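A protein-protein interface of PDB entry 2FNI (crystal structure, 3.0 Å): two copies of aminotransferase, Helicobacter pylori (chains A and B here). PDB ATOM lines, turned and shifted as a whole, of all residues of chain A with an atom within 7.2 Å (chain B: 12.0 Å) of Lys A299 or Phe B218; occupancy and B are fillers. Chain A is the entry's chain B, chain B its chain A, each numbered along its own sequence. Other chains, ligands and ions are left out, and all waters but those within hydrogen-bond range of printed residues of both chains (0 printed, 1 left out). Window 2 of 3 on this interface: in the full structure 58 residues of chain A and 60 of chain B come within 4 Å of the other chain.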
ATOM      1  N   MET A 290     -31.438   3.012 -12.712  1.00  0.00           N
ATOM      2  CA  MET A 290     -30.753   4.205 -13.197  1.00  0.00           C
ATOM      3  C   MET A 290     -29.734   3.857 -14.263  1.00  0.00           C
ATOM      4  O   MET A 290     -29.183   2.756 -14.250  1.00  0.00           O
ATOM      5  CB  MET A 290     -30.004   4.866 -12.051  1.00  0.00           C
ATOM      6  CG  MET A 290     -30.872   5.317 -10.906  1.00  0.00           C
ATOM      7  SD  MET A 290     -29.976   6.400  -9.773  1.00  0.00           S
ATOM      8  CE  MET A 290     -28.359   5.629  -9.690  1.00  0.00           C
ATOM      9  N   PHE A 294     -25.725   8.042 -13.656  1.00  0.00           N
ATOM     10  CA  PHE A 294     -26.198   8.576 -12.373  1.00  0.00           C
ATOM     11  C   PHE A 294     -25.612   7.884 -11.163  1.00  0.00           C
ATOM     12  O   PHE A 294     -25.732   8.388 -10.047  1.00  0.00           O
ATOM     13  CB  PHE A 294     -27.720   8.522 -12.283  1.00  0.00           C
ATOM     14  CG  PHE A 294     -28.401   9.487 -13.192  1.00  0.00           C
ATOM     15  CD1 PHE A 294     -28.490  10.835 -12.856  1.00  0.00           C
ATOM     16  CD2 PHE A 294     -28.939   9.060 -14.392  1.00  0.00           C
ATOM     17  CE1 PHE A 294     -29.118  11.744 -13.703  1.00  0.00           C
ATOM     18  CE2 PHE A 294     -29.570   9.966 -15.256  1.00  0.00           C
ATOM     19  CZ  PHE A 294     -29.662  11.311 -14.908  1.00  0.00           C
ATOM     20  N   PHE A 295     -24.989   6.730 -11.395  1.00  0.00           N
ATOM     21  CA  PHE A 295     -24.448   5.891 -10.328  1.00  0.00           C
ATOM     22  C   PHE A 295     -23.721   6.665  -9.241  1.00  0.00           C
ATOM     23  O   PHE A 295     -24.067   6.561  -8.059  1.00  0.00           O
ATOM     24  CB  PHE A 295     -23.476   4.879 -10.911  1.00  0.00           C
ATOM     25  CG  PHE A 295     -24.134   3.686 -11.512  1.00  0.00           C
ATOM     26  CD1 PHE A 295     -23.396   2.539 -11.773  1.00  0.00           C
ATOM     27  CD2 PHE A 295     -25.485   3.700 -11.806  1.00  0.00           C
ATOM     28  CE1 PHE A 295     -23.992   1.435 -12.333  1.00  0.00           C
ATOM     29  CE2 PHE A 295     -26.091   2.606 -12.366  1.00  0.00           C
ATOM     30  CZ  PHE A 295     -25.346   1.466 -12.630  1.00  0.00           C
ATOM     31  N   THR A 296     -22.710   7.437  -9.650  1.00  0.00           N
ATOM     32  CA  THR A 296     -21.760   8.064  -8.707  1.00  0.00           C
ATOM     33  C   THR A 296     -22.397   9.130  -7.805  1.00  0.00           C
ATOM     34  O   THR A 296     -21.808   9.532  -6.800  1.00  0.00           O
ATOM     35  CB  THR A 296     -20.497   8.620  -9.426  1.00  0.00           C
ATOM     36  OG1 THR A 296     -20.692   9.997  -9.763  1.00  0.00           O
ATOM     37  CG2 THR A 296     -20.197   7.800 -10.693  1.00  0.00           C
ATOM     38  N   CYS A 297     -23.604   9.570  -8.140  1.00  0.00           N
ATOM     39  CA  CYS A 297     -24.302  10.475  -7.254  1.00  0.00           C
ATOM     40  C   CYS A 297     -25.670   9.910  -6.810  1.00  0.00           C
ATOM     41  O   CYS A 297     -26.676  10.634  -6.674  1.00  0.00           O
ATOM     42  CB  CYS A 297     -24.400  11.862  -7.894  1.00  0.00           C
ATOM     43  SG  CYS A 297     -25.675  12.036  -9.128  1.00  0.00           S
ATOM     44  N   LYS A 298     -25.687   8.602  -6.559  1.00  0.00           N
ATOM     45  CA  LYS A 298     -26.916   7.941  -6.158  1.00  0.00           C
ATOM     46  C   LYS A 298     -27.406   8.494  -4.832  1.00  0.00           C
ATOM     47  O   LYS A 298     -28.589   8.831  -4.680  1.00  0.00           O
ATOM     48  CB  LYS A 298     -26.728   6.430  -6.043  1.00  0.00           C
ATOM     49  CG  LYS A 298     -28.018   5.731  -5.626  1.00  0.00           C
ATOM     50  CD  LYS A 298     -27.991   4.251  -5.926  1.00  0.00           C
ATOM     51  CE  LYS A 298     -29.369   3.632  -5.830  1.00  0.00           C
ATOM     52  NZ  LYS A 298     -29.258   2.165  -5.975  1.00  0.00           N
ATOM     53  N   LYS A 299     -26.475   8.582  -3.884  1.00  0.00           N
ATOM     54  CA  LYS A 299     -26.779   9.020  -2.527  1.00  0.00           C
ATOM     55  C   LYS A 299     -27.579  10.328  -2.524  1.00  0.00           C
ATOM     56  O   LYS A 299     -28.607  10.434  -1.848  1.00  0.00           O
ATOM     57  CB  LYS A 299     -25.482   9.166  -1.718  1.00  0.00           C
ATOM     58  CG  LYS A 299     -25.671   9.158  -0.203  1.00  0.00           C
ATOM     59  CD  LYS A 299     -26.052   7.767   0.312  1.00  0.00           C
ATOM     60  CE  LYS A 299     -26.444   7.807   1.800  1.00  0.00           C
ATOM     61  NZ  LYS A 299     -25.403   8.475   2.647  1.00  0.00           N
ATOM     62  N   LEU A 300     -27.113  11.308  -3.299  1.00  0.00           N
ATOM     63  CA  LEU A 300     -27.749  12.624  -3.365  1.00  0.00           C
ATOM     64  C   LEU A 300     -29.140  12.561  -3.953  1.00  0.00           C
ATOM     65  O   LEU A 300     -29.990  13.387  -3.638  1.00  0.00           O
ATOM     66  CB  LEU A 300     -26.909  13.575  -4.205  1.00  0.00           C
ATOM     67  CG  LEU A 300     -25.479  13.788  -3.712  1.00  0.00           C
ATOM     68  CD1 LEU A 300     -24.742  14.797  -4.604  1.00  0.00           C
ATOM     69  CD2 LEU A 300     -25.476  14.226  -2.241  1.00  0.00           C
ATOM     70  N   ILE A 301     -29.359  11.583  -4.824  1.00  0.00           N
ATOM     71  CA  ILE A 301     -30.657  11.376  -5.456  1.00  0.00           C
ATOM     72  C   ILE A 301     -31.662  10.829  -4.446  1.00  0.00           C
ATOM     73  O   ILE A 301     -32.784  11.336  -4.317  1.00  0.00           O
ATOM     74  CB  ILE A 301     -30.528  10.433  -6.671  1.00  0.00           C
ATOM     75  CG1 ILE A 301     -29.733  11.123  -7.781  1.00  0.00           C
ATOM     76  CG2 ILE A 301     -31.893  10.021  -7.189  1.00  0.00           C
ATOM     77  CD1 ILE A 301     -29.642  10.317  -9.048  1.00  0.00           C
ATOM     78  N   LEU A 302     -31.244   9.799  -3.720  1.00  0.00           N
ATOM     79  CA  LEU A 302     -32.058   9.242  -2.643  1.00  0.00           C
ATOM     80  C   LEU A 302     -32.454  10.311  -1.628  1.00  0.00           C
ATOM     81  O   LEU A 302     -33.623  10.399  -1.230  1.00  0.00           O
ATOM     82  CB  LEU A 302     -31.315   8.103  -1.949  1.00  0.00           C
ATOM     83  CG  LEU A 302     -31.080   6.908  -2.871  1.00  0.00           C
ATOM     84  CD1 LEU A 302     -30.478   5.729  -2.116  1.00  0.00           C
ATOM     85  CD2 LEU A 302     -32.388   6.524  -3.555  1.00  0.00           C
ATOM     86  N   GLU A 303     -31.479  11.122  -1.214  1.00  0.00           N
ATOM     87  CA  GLU A 303     -31.738  12.208  -0.272  1.00  0.00           C
ATOM     88  C   GLU A 303     -32.700  13.221  -0.873  1.00  0.00           C
ATOM     89  O   GLU A 303     -33.602  13.702  -0.185  1.00  0.00           O
ATOM     90  CB  GLU A 303     -30.445  12.897   0.165  1.00  0.00           C
ATOM     91  CG  GLU A 303     -29.625  12.102   1.177  1.00  0.00           C
ATOM     92  CD  GLU A 303     -28.178  12.583   1.251  1.00  0.00           C
ATOM     93  OE1 GLU A 303     -27.933  13.758   0.877  1.00  0.00           O
ATOM     94  OE2 GLU A 303     -27.291  11.789   1.672  1.00  0.00           O
ATOM     95  N   SER A 304     -32.510  13.536  -2.153  1.00  0.00           N
ATOM     96  CA  SER A 304     -33.383  14.488  -2.829  1.00  0.00           C
ATOM     97  C   SER A 304     -34.798  13.950  -2.837  1.00  0.00           C
ATOM     98  O   SER A 304     -35.747  14.684  -2.560  1.00  0.00           O
ATOM     99  CB  SER A 304     -32.925  14.740  -4.262  1.00  0.00           C
ATOM    100  OG  SER A 304     -33.956  15.371  -5.004  1.00  0.00           O
ATOM    101  N   LEU A 305     -34.939  12.667  -3.160  1.00  0.00           N
ATOM    102  CA  LEU A 305     -36.256  12.029  -3.180  1.00  0.00           C
ATOM    103  C   LEU A 305     -36.894  12.099  -1.794  1.00  0.00           C
ATOM    104  O   LEU A 305     -38.059  12.488  -1.649  1.00  0.00           O
ATOM    105  CB  LEU A 305     -36.149  10.566  -3.637  1.00  0.00           C
ATOM    106  CG  LEU A 305     -35.959  10.238  -5.118  1.00  0.00           C
ATOM    107  CD1 LEU A 305     -35.628   8.780  -5.258  1.00  0.00           C
ATOM    108  CD2 LEU A 305     -37.201  10.574  -5.913  1.00  0.00           C
ATOM    109  N   HIS A 306     -36.111  11.725  -0.779  1.00  0.00           N
ATOM    110  CA  HIS A 306     -36.585  11.710   0.596  1.00  0.00           C
ATOM    111  C   HIS A 306     -37.061  13.074   1.031  1.00  0.00           C
ATOM    112  O   HIS A 306     -38.025  13.172   1.781  1.00  0.00           O
ATOM    113  CB  HIS A 306     -35.520  11.163   1.538  1.00  0.00           C
ATOM    114  CG  HIS A 306     -35.558   9.675   1.658  1.00  0.00           C
ATOM    115  ND1 HIS A 306     -35.745   9.030   2.860  1.00  0.00           N
ATOM    116  CD2 HIS A 306     -35.479   8.705   0.716  1.00  0.00           C
ATOM    117  CE1 HIS A 306     -35.754   7.724   2.658  1.00  0.00           C
ATOM    118  NE2 HIS A 306     -35.598   7.501   1.365  1.00  0.00           N
ATOM    119  N   ILE A 310     -40.774  11.073  -0.715  1.00  0.00           N
ATOM    120  CA  ILE A 310     -40.726   9.778  -1.352  1.00  0.00           C
ATOM    121  C   ILE A 310     -39.657   8.936  -0.685  1.00  0.00           C
ATOM    122  O   ILE A 310     -38.507   8.945  -1.098  1.00  0.00           O
ATOM    123  CB  ILE A 310     -40.415   9.925  -2.831  1.00  0.00           C
ATOM    124  CG1 ILE A 310     -41.540  10.695  -3.507  1.00  0.00           C
ATOM    125  CG2 ILE A 310     -40.250   8.572  -3.470  1.00  0.00           C
ATOM    126  CD1 ILE A 310     -41.185  11.198  -4.877  1.00  0.00           C
ATOM    127  N   LEU A 311     -40.038   8.215   0.361  1.00  0.00           N
ATOM    128  CA  LEU A 311     -39.078   7.430   1.128  1.00  0.00           C
ATOM    129  C   LEU A 311     -38.681   6.183   0.362  1.00  0.00           C
ATOM    130  O   LEU A 311     -39.122   5.085   0.695  1.00  0.00           O
ATOM    131  CB  LEU A 311     -39.659   7.037   2.495  1.00  0.00           C
ATOM    132  CG  LEU A 311     -40.239   8.108   3.447  1.00  0.00           C
ATOM    133  CD1 LEU A 311     -40.831   7.460   4.704  1.00  0.00           C
ATOM    134  CD2 LEU A 311     -39.210   9.182   3.837  1.00  0.00           C
ATOM    135  N   ALA A 312     -37.849   6.366  -0.663  1.00  0.00           N
ATOM    136  CA  ALA A 312     -37.356   5.257  -1.485  1.00  0.00           C
ATOM    137  C   ALA A 312     -36.355   4.383  -0.732  1.00  0.00           C
ATOM    138  O   ALA A 312     -35.886   4.730   0.354  1.00  0.00           O
ATOM    139  CB  ALA A 312     -36.744   5.774  -2.783  1.00  0.00           C
ATOM    140  N   GLN A 313     -36.023   3.246  -1.326  1.00  0.00           N
ATOM    141  CA  GLN A 313     -35.180   2.269  -0.674  1.00  0.00           C
ATOM    142  C   GLN A 313     -34.443   1.499  -1.766  1.00  0.00           C
ATOM    143  O   GLN A 313     -34.824   1.574  -2.934  1.00  0.00           O
ATOM    144  CB  GLN A 313     -36.066   1.343   0.164  1.00  0.00           C
ATOM    145  CG  GLN A 313     -35.431   0.818   1.430  1.00  0.00           C
ATOM    146  CD  GLN A 313     -34.755   1.914   2.209  1.00  0.00           C
ATOM    147  OE1 GLN A 313     -33.535   2.084   2.124  1.00  0.00           O
ATOM    148  NE2 GLN A 313     -35.542   2.689   2.946  1.00  0.00           N
ATOM    149  N   VAL A 314     -33.384   0.781  -1.407  1.00  0.00           N
ATOM    150  CA  VAL A 314     -32.660  -0.027  -2.387  1.00  0.00           C
ATOM    151  C   VAL A 314     -32.723  -1.512  -2.037  1.00  0.00           C
ATOM    152  O   VAL A 314     -32.383  -1.902  -0.924  1.00  0.00           O
ATOM    153  CB  VAL A 314     -31.170   0.371  -2.485  1.00  0.00           C
ATOM    154  CG1 VAL A 314     -30.439  -0.537  -3.482  1.00  0.00           C
ATOM    155  CG2 VAL A 314     -31.023   1.828  -2.868  1.00  0.00           C
ATOM    156  N   HIS A 315     -33.155  -2.339  -2.983  1.00  0.00           N
ATOM    157  CA  HIS A 315     -33.107  -3.783  -2.804  1.00  0.00           C
ATOM    158  C   HIS A 315     -32.335  -4.358  -3.972  1.00  0.00           C
ATOM    159  O   HIS A 315     -32.799  -4.279  -5.100  1.00  0.00           O
ATOM    160  CB  HIS A 315     -34.516  -4.376  -2.769  1.00  0.00           C
ATOM    161  CG  HIS A 315     -35.428  -3.699  -1.798  1.00  0.00           C
ATOM    162  ND1 HIS A 315     -36.308  -2.707  -2.172  1.00  0.00           N
ATOM    163  CD2 HIS A 315     -35.586  -3.857  -0.464  1.00  0.00           C
ATOM    164  CE1 HIS A 315     -36.972  -2.286  -1.110  1.00  0.00           C
ATOM    165  NE2 HIS A 315     -36.552  -2.966  -0.059  1.00  0.00           N
ATOM    166  N   LYS A 317     -28.419  -4.541  -1.350  1.00  0.00           N
ATOM    167  CA  LYS A 317     -26.974  -4.521  -1.293  1.00  0.00           C
ATOM    168  C   LYS A 317     -26.499  -5.954  -1.495  1.00  0.00           C
ATOM    169  O   LYS A 317     -26.993  -6.864  -0.835  1.00  0.00           O
ATOM    170  CB  LYS A 317     -26.536  -3.987   0.064  1.00  0.00           C
ATOM    171  CG  LYS A 317     -25.058  -4.026   0.325  1.00  0.00           C
ATOM    172  CD  LYS A 317     -24.747  -3.361   1.650  1.00  0.00           C
ATOM    173  CE  LYS A 317     -23.256  -3.285   1.881  1.00  0.00           C
ATOM    174  NZ  LYS A 317     -22.950  -2.607   3.158  1.00  0.00           N
ATOM    175  N   TYR A 341     -27.113  -3.254  -8.134  1.00  0.00           N
ATOM    176  CA  TYR A 341     -27.162  -2.561  -6.853  1.00  0.00           C
ATOM    177  C   TYR A 341     -27.117  -1.036  -7.026  1.00  0.00           C
ATOM    178  O   TYR A 341     -28.021  -0.328  -6.576  1.00  0.00           O
ATOM    179  CB  TYR A 341     -26.032  -3.053  -5.940  1.00  0.00           C
ATOM    180  CG  TYR A 341     -25.904  -2.334  -4.611  1.00  0.00           C
ATOM    181  CD1 TYR A 341     -27.004  -2.136  -3.795  1.00  0.00           C
ATOM    182  CD2 TYR A 341     -24.667  -1.879  -4.166  1.00  0.00           C
ATOM    183  CE1 TYR A 341     -26.879  -1.486  -2.577  1.00  0.00           C
ATOM    184  CE2 TYR A 341     -24.528  -1.237  -2.952  1.00  0.00           C
ATOM    185  CZ  TYR A 341     -25.635  -1.045  -2.160  1.00  0.00           C
ATOM    186  OH  TYR A 341     -25.498  -0.405  -0.948  1.00  0.00           O
ATOM    187  N   PHE A 372     -30.385  16.842 -11.543  1.00  0.00           N
ATOM    188  CA  PHE A 372     -28.952  16.476 -11.630  1.00  0.00           C
ATOM    189  C   PHE A 372     -28.415  16.450 -13.078  1.00  0.00           C
ATOM    190  O   PHE A 372     -28.078  15.374 -13.598  1.00  0.00           O
ATOM    191  CB  PHE A 372     -28.712  15.100 -11.006  1.00  0.00           C
ATOM    192  CG  PHE A 372     -28.988  15.036  -9.537  1.00  0.00           C
ATOM    193  CD1 PHE A 372     -30.283  14.881  -9.063  1.00  0.00           C
ATOM    194  CD2 PHE A 372     -27.942  15.107  -8.622  1.00  0.00           C
ATOM    195  CE1 PHE A 372     -30.533  14.815  -7.702  1.00  0.00           C
ATOM    196  CE2 PHE A 372     -28.184  15.048  -7.255  1.00  0.00           C
ATOM    197  CZ  PHE A 372     -29.482  14.898  -6.794  1.00  0.00           C
ATOM    198  N   MET B 212     -28.500  -7.093  11.667  1.00  0.00           N
ATOM    199  CA  MET B 212     -28.460  -5.821  10.933  1.00  0.00           C
ATOM    200  C   MET B 212     -28.146  -4.604  11.806  1.00  0.00           C
ATOM    201  O   MET B 212     -28.835  -4.338  12.784  1.00  0.00           O
ATOM    202  CB  MET B 212     -29.783  -5.594  10.197  1.00  0.00           C
ATOM    203  CG  MET B 212     -29.752  -4.478   9.178  1.00  0.00           C
ATOM    204  SD  MET B 212     -28.675  -4.890   7.805  1.00  0.00           S
ATOM    205  CE  MET B 212     -29.637  -6.154   6.971  1.00  0.00           C
ATOM    206  N   LEU B 213     -27.097  -3.876  11.439  1.00  0.00           N
ATOM    207  CA  LEU B 213     -26.743  -2.603  12.063  1.00  0.00           C
ATOM    208  C   LEU B 213     -27.028  -1.504  11.052  1.00  0.00           C
ATOM    209  O   LEU B 213     -26.757  -1.694   9.865  1.00  0.00           O
ATOM    210  CB  LEU B 213     -25.255  -2.595  12.380  1.00  0.00           C
ATOM    211  CG  LEU B 213     -24.759  -3.591  13.430  1.00  0.00           C
ATOM    212  CD1 LEU B 213     -23.499  -4.345  12.972  1.00  0.00           C
ATOM    213  CD2 LEU B 213     -24.522  -2.863  14.758  1.00  0.00           C
ATOM    214  N   LYS B 214     -27.565  -0.365  11.493  1.00  0.00           N
ATOM    215  CA  LYS B 214     -27.920   0.711  10.544  1.00  0.00           C
ATOM    216  C   LYS B 214     -26.738   1.640  10.219  1.00  0.00           C
ATOM    217  O   LYS B 214     -25.780   1.736  10.987  1.00  0.00           O
ATOM    218  CB  LYS B 214     -29.133   1.545  11.016  1.00  0.00           C
ATOM    219  CG  LYS B 214     -30.534   0.854  11.000  1.00  0.00           C
ATOM    220  CD  LYS B 214     -30.651  -0.487  10.190  1.00  0.00           C
ATOM    221  CE  LYS B 214     -30.378  -0.380   8.656  1.00  0.00           C
ATOM    222  NZ  LYS B 214     -31.106   0.721   7.940  1.00  0.00           N
ATOM    223  N   LYS B 215     -26.801   2.300   9.062  1.00  0.00           N
ATOM    224  CA  LYS B 215     -25.843   3.356   8.717  1.00  0.00           C
ATOM    225  C   LYS B 215     -26.591   4.657   8.431  1.00  0.00           C
ATOM    226  O   LYS B 215     -26.311   5.693   9.030  1.00  0.00           O
ATOM    227  CB  LYS B 215     -24.998   2.979   7.498  1.00  0.00           C
ATOM    228  CG  LYS B 215     -23.869   2.016   7.775  1.00  0.00           C
ATOM    229  CD  LYS B 215     -23.062   1.823   6.507  1.00  0.00           C
ATOM    230  CE  LYS B 215     -21.987   0.762   6.688  1.00  0.00           C
ATOM    231  NZ  LYS B 215     -21.255   0.527   5.409  1.00  0.00           N
ATOM    232  N   ASP B 216     -27.538   4.582   7.502  1.00  0.00           N
ATOM    233  CA  ASP B 216     -28.385   5.698   7.104  1.00  0.00           C
ATOM    234  C   ASP B 216     -29.688   5.025   6.726  1.00  0.00           C
ATOM    235  O   ASP B 216     -29.811   3.805   6.896  1.00  0.00           O
ATOM    236  CB  ASP B 216     -27.777   6.402   5.901  1.00  0.00           C
ATOM    237  CG  ASP B 216     -27.068   5.437   4.974  1.00  0.00           C
ATOM    238  OD1 ASP B 216     -25.848   5.233   5.146  1.00  0.00           O
ATOM    239  OD2 ASP B 216     -27.736   4.856   4.096  1.00  0.00           O
ATOM    240  N   PHE B 217     -30.661   5.761   6.199  1.00  0.00           N
ATOM    241  CA  PHE B 217     -31.926   5.083   5.908  1.00  0.00           C
ATOM    242  C   PHE B 217     -31.782   4.053   4.778  1.00  0.00           C
ATOM    243  O   PHE B 217     -32.694   3.255   4.546  1.00  0.00           O
ATOM    244  CB  PHE B 217     -33.099   6.058   5.672  1.00  0.00           C
ATOM    245  CG  PHE B 217     -34.473   5.406   5.820  1.00  0.00           C
ATOM    246  CD1 PHE B 217     -34.817   4.718   6.999  1.00  0.00           C
ATOM    247  CD2 PHE B 217     -35.414   5.475   4.783  1.00  0.00           C
ATOM    248  CE1 PHE B 217     -36.075   4.108   7.143  1.00  0.00           C
ATOM    249  CE2 PHE B 217     -36.683   4.873   4.915  1.00  0.00           C
ATOM    250  CZ  PHE B 217     -37.010   4.186   6.101  1.00  0.00           C
ATOM    251  N   PHE B 218     -30.621   4.034   4.123  1.00  0.00           N
ATOM    252  CA  PHE B 218     -30.456   3.248   2.898  1.00  0.00           C
ATOM    253  C   PHE B 218     -29.527   2.033   2.974  1.00  0.00           C
ATOM    254  O   PHE B 218     -29.554   1.182   2.080  1.00  0.00           O
ATOM    255  CB  PHE B 218     -30.010   4.157   1.757  1.00  0.00           C
ATOM    256  CG  PHE B 218     -30.735   5.462   1.721  1.00  0.00           C
ATOM    257  CD1 PHE B 218     -30.077   6.648   2.017  1.00  0.00           C
ATOM    258  CD2 PHE B 218     -32.086   5.503   1.413  1.00  0.00           C
ATOM    259  CE1 PHE B 218     -30.758   7.859   1.987  1.00  0.00           C
ATOM    260  CE2 PHE B 218     -32.771   6.704   1.384  1.00  0.00           C
ATOM    261  CZ  PHE B 218     -32.112   7.883   1.671  1.00  0.00           C
ATOM    262  N   GLU B 219     -28.709   1.944   4.017  1.00  0.00           N
ATOM    263  CA  GLU B 219     -27.725   0.867   4.082  1.00  0.00           C
ATOM    264  C   GLU B 219     -27.542   0.295   5.480  1.00  0.00           C
ATOM    265  O   GLU B 219     -27.725   0.985   6.481  1.00  0.00           O
ATOM    266  CB  GLU B 219     -26.373   1.334   3.532  1.00  0.00           C
ATOM    267  CG  GLU B 219     -25.396   0.198   3.268  1.00  0.00           C
ATOM    268  CD  GLU B 219     -24.104   0.676   2.644  1.00  0.00           C
ATOM    269  OE1 GLU B 219     -23.205  -0.166   2.410  1.00  0.00           O
ATOM    270  OE2 GLU B 219     -23.994   1.892   2.383  1.00  0.00           O
ATOM    271  N   GLY B 220     -27.175  -0.977   5.536  1.00  0.00           N
ATOM    272  CA  GLY B 220     -26.893  -1.624   6.807  1.00  0.00           C
ATOM    273  C   GLY B 220     -25.544  -2.323   6.829  1.00  0.00           C
ATOM    274  O   GLY B 220     -24.781  -2.290   5.854  1.00  0.00           O
ATOM    275  N   GLU B 221     -25.246  -2.964   7.952  1.00  0.00           N
ATOM    276  CA  GLU B 221     -24.010  -3.716   8.072  1.00  0.00           C
ATOM    277  C   GLU B 221     -24.255  -4.992   8.854  1.00  0.00           C
ATOM    278  O   GLU B 221     -24.966  -4.990   9.854  1.00  0.00           O
ATOM    279  CB  GLU B 221     -22.931  -2.878   8.756  1.00  0.00           C
ATOM    280  CG  GLU B 221     -21.594  -3.567   8.785  1.00  0.00           C
ATOM    281  CD  GLU B 221     -21.185  -4.038   7.412  1.00  0.00           C
ATOM    282  OE1 GLU B 221     -20.701  -3.198   6.630  1.00  0.00           O
ATOM    283  OE2 GLU B 221     -21.353  -5.238   7.107  1.00  0.00           O
ATOM    284  N   VAL B 222     -23.673  -6.089   8.395  1.00  0.00           N
ATOM    285  CA  VAL B 222     -23.865  -7.350   9.087  1.00  0.00           C
ATOM    286  C   VAL B 222     -22.528  -7.982   9.452  1.00  0.00           C
ATOM    287  O   VAL B 222     -21.793  -8.427   8.568  1.00  0.00           O
ATOM    288  CB  VAL B 222     -24.730  -8.322   8.256  1.00  0.00           C
ATOM    289  CG1 VAL B 222     -24.823  -9.671   8.940  1.00  0.00           C
ATOM    290  CG2 VAL B 222     -26.122  -7.741   8.049  1.00  0.00           C
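Of the 23 printed residues of chain A, 6 touch a printed residue of chain B. Printed residues of chain A that touch a printed residue of chain B: Lys A299, Leu A302, His A306, Ala A312, Gln A313 and Lys A317. Hydrophobic or aromatic side chains of chain A that line the printed part of chain B: Leu A302 and His A306. Hydrophobic or aromatic side chains of chain B that line the printed part of chain A: Phe B217 and Phe B218. Among the printed residues, Asp or Glu carboxylates within 4 Å of a Lys or Arg side-chain nitrogen of the other chain: Lys A317 with Glu B219.
OD2 of Asp B216 touches CE of Lys A299 (3.96 Å). Lys A299 touches Phe B218 (CE to CD1, 3.8 Å). Leu A302 touches Phe B218 (CB to CZ, 3.7 Å). Phe B217 touches His A306. NE2 of His A306 touches CE2 of Phe B218, 2.9 Å away. CE2 of Phe B218 touches O of Ala A312, 3.8 Å away. Gln A313 touches Phe B218 (OE1 to CA, 3.4 Å).
NZ of Lys B215 is in salt-bridge range of OE1 of Glu B219, 3.6 Å away. The side-chain carboxylate of Asp B216 sits close to the backbone NH of Phe B218, at 3.0 Å. OD2 of Asp B216 lies within hydrogen-bond range of N of Glu B219, at 3.1 Å. OE2 of Glu A303 lies within salt-bridge range of NZ of Lys A299, at 3.9 Å. A ring nitrogen (NE2) of His A306 lies within hydrogen-bond range of the backbone carbonyl oxygen (O) of Ala A312 (3.0 Å).
The side-chain amide oxygen (OE1) of Gln A313 sits close to the backbone carbonyl oxygen (O) of Phe B217 (2.8 Å). The side-chain amino group (NZ) of Lys A317 lies within salt-bridge range of the side-chain carboxylate (OE1) of Glu B219 (2.6 Å). The backbone carbonyl oxygen of Gly B220 lies within hydrogen-bond range of the side-chain amino group of Lys A317.
Of chain B, only Asp B216 and Phe B218 come within 4 Å of Lys A299. Phe B218 touches five residues of chain A. No residue of chain B comes within 4 Å of Cys A297. No residue of chain B comes within 4 Å of Lys A298. No residue of chain B comes within 4 Å of Leu A300. Of chain B, only Phe B218 (3.7 Å) comes within 4 Å of Leu A302. His A306 touches two residues of chain B. No residue of chain B comes within 4 Å of Val A314. Printed residues of chain A within 4 Å of Asp B216: Lys A299 (3.96 Å). Of the printed residues of chain A, Phe B217 touches His A306 (3.1 Å) and Gln A313 (2.8 Å).
No position is printed for both chains.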
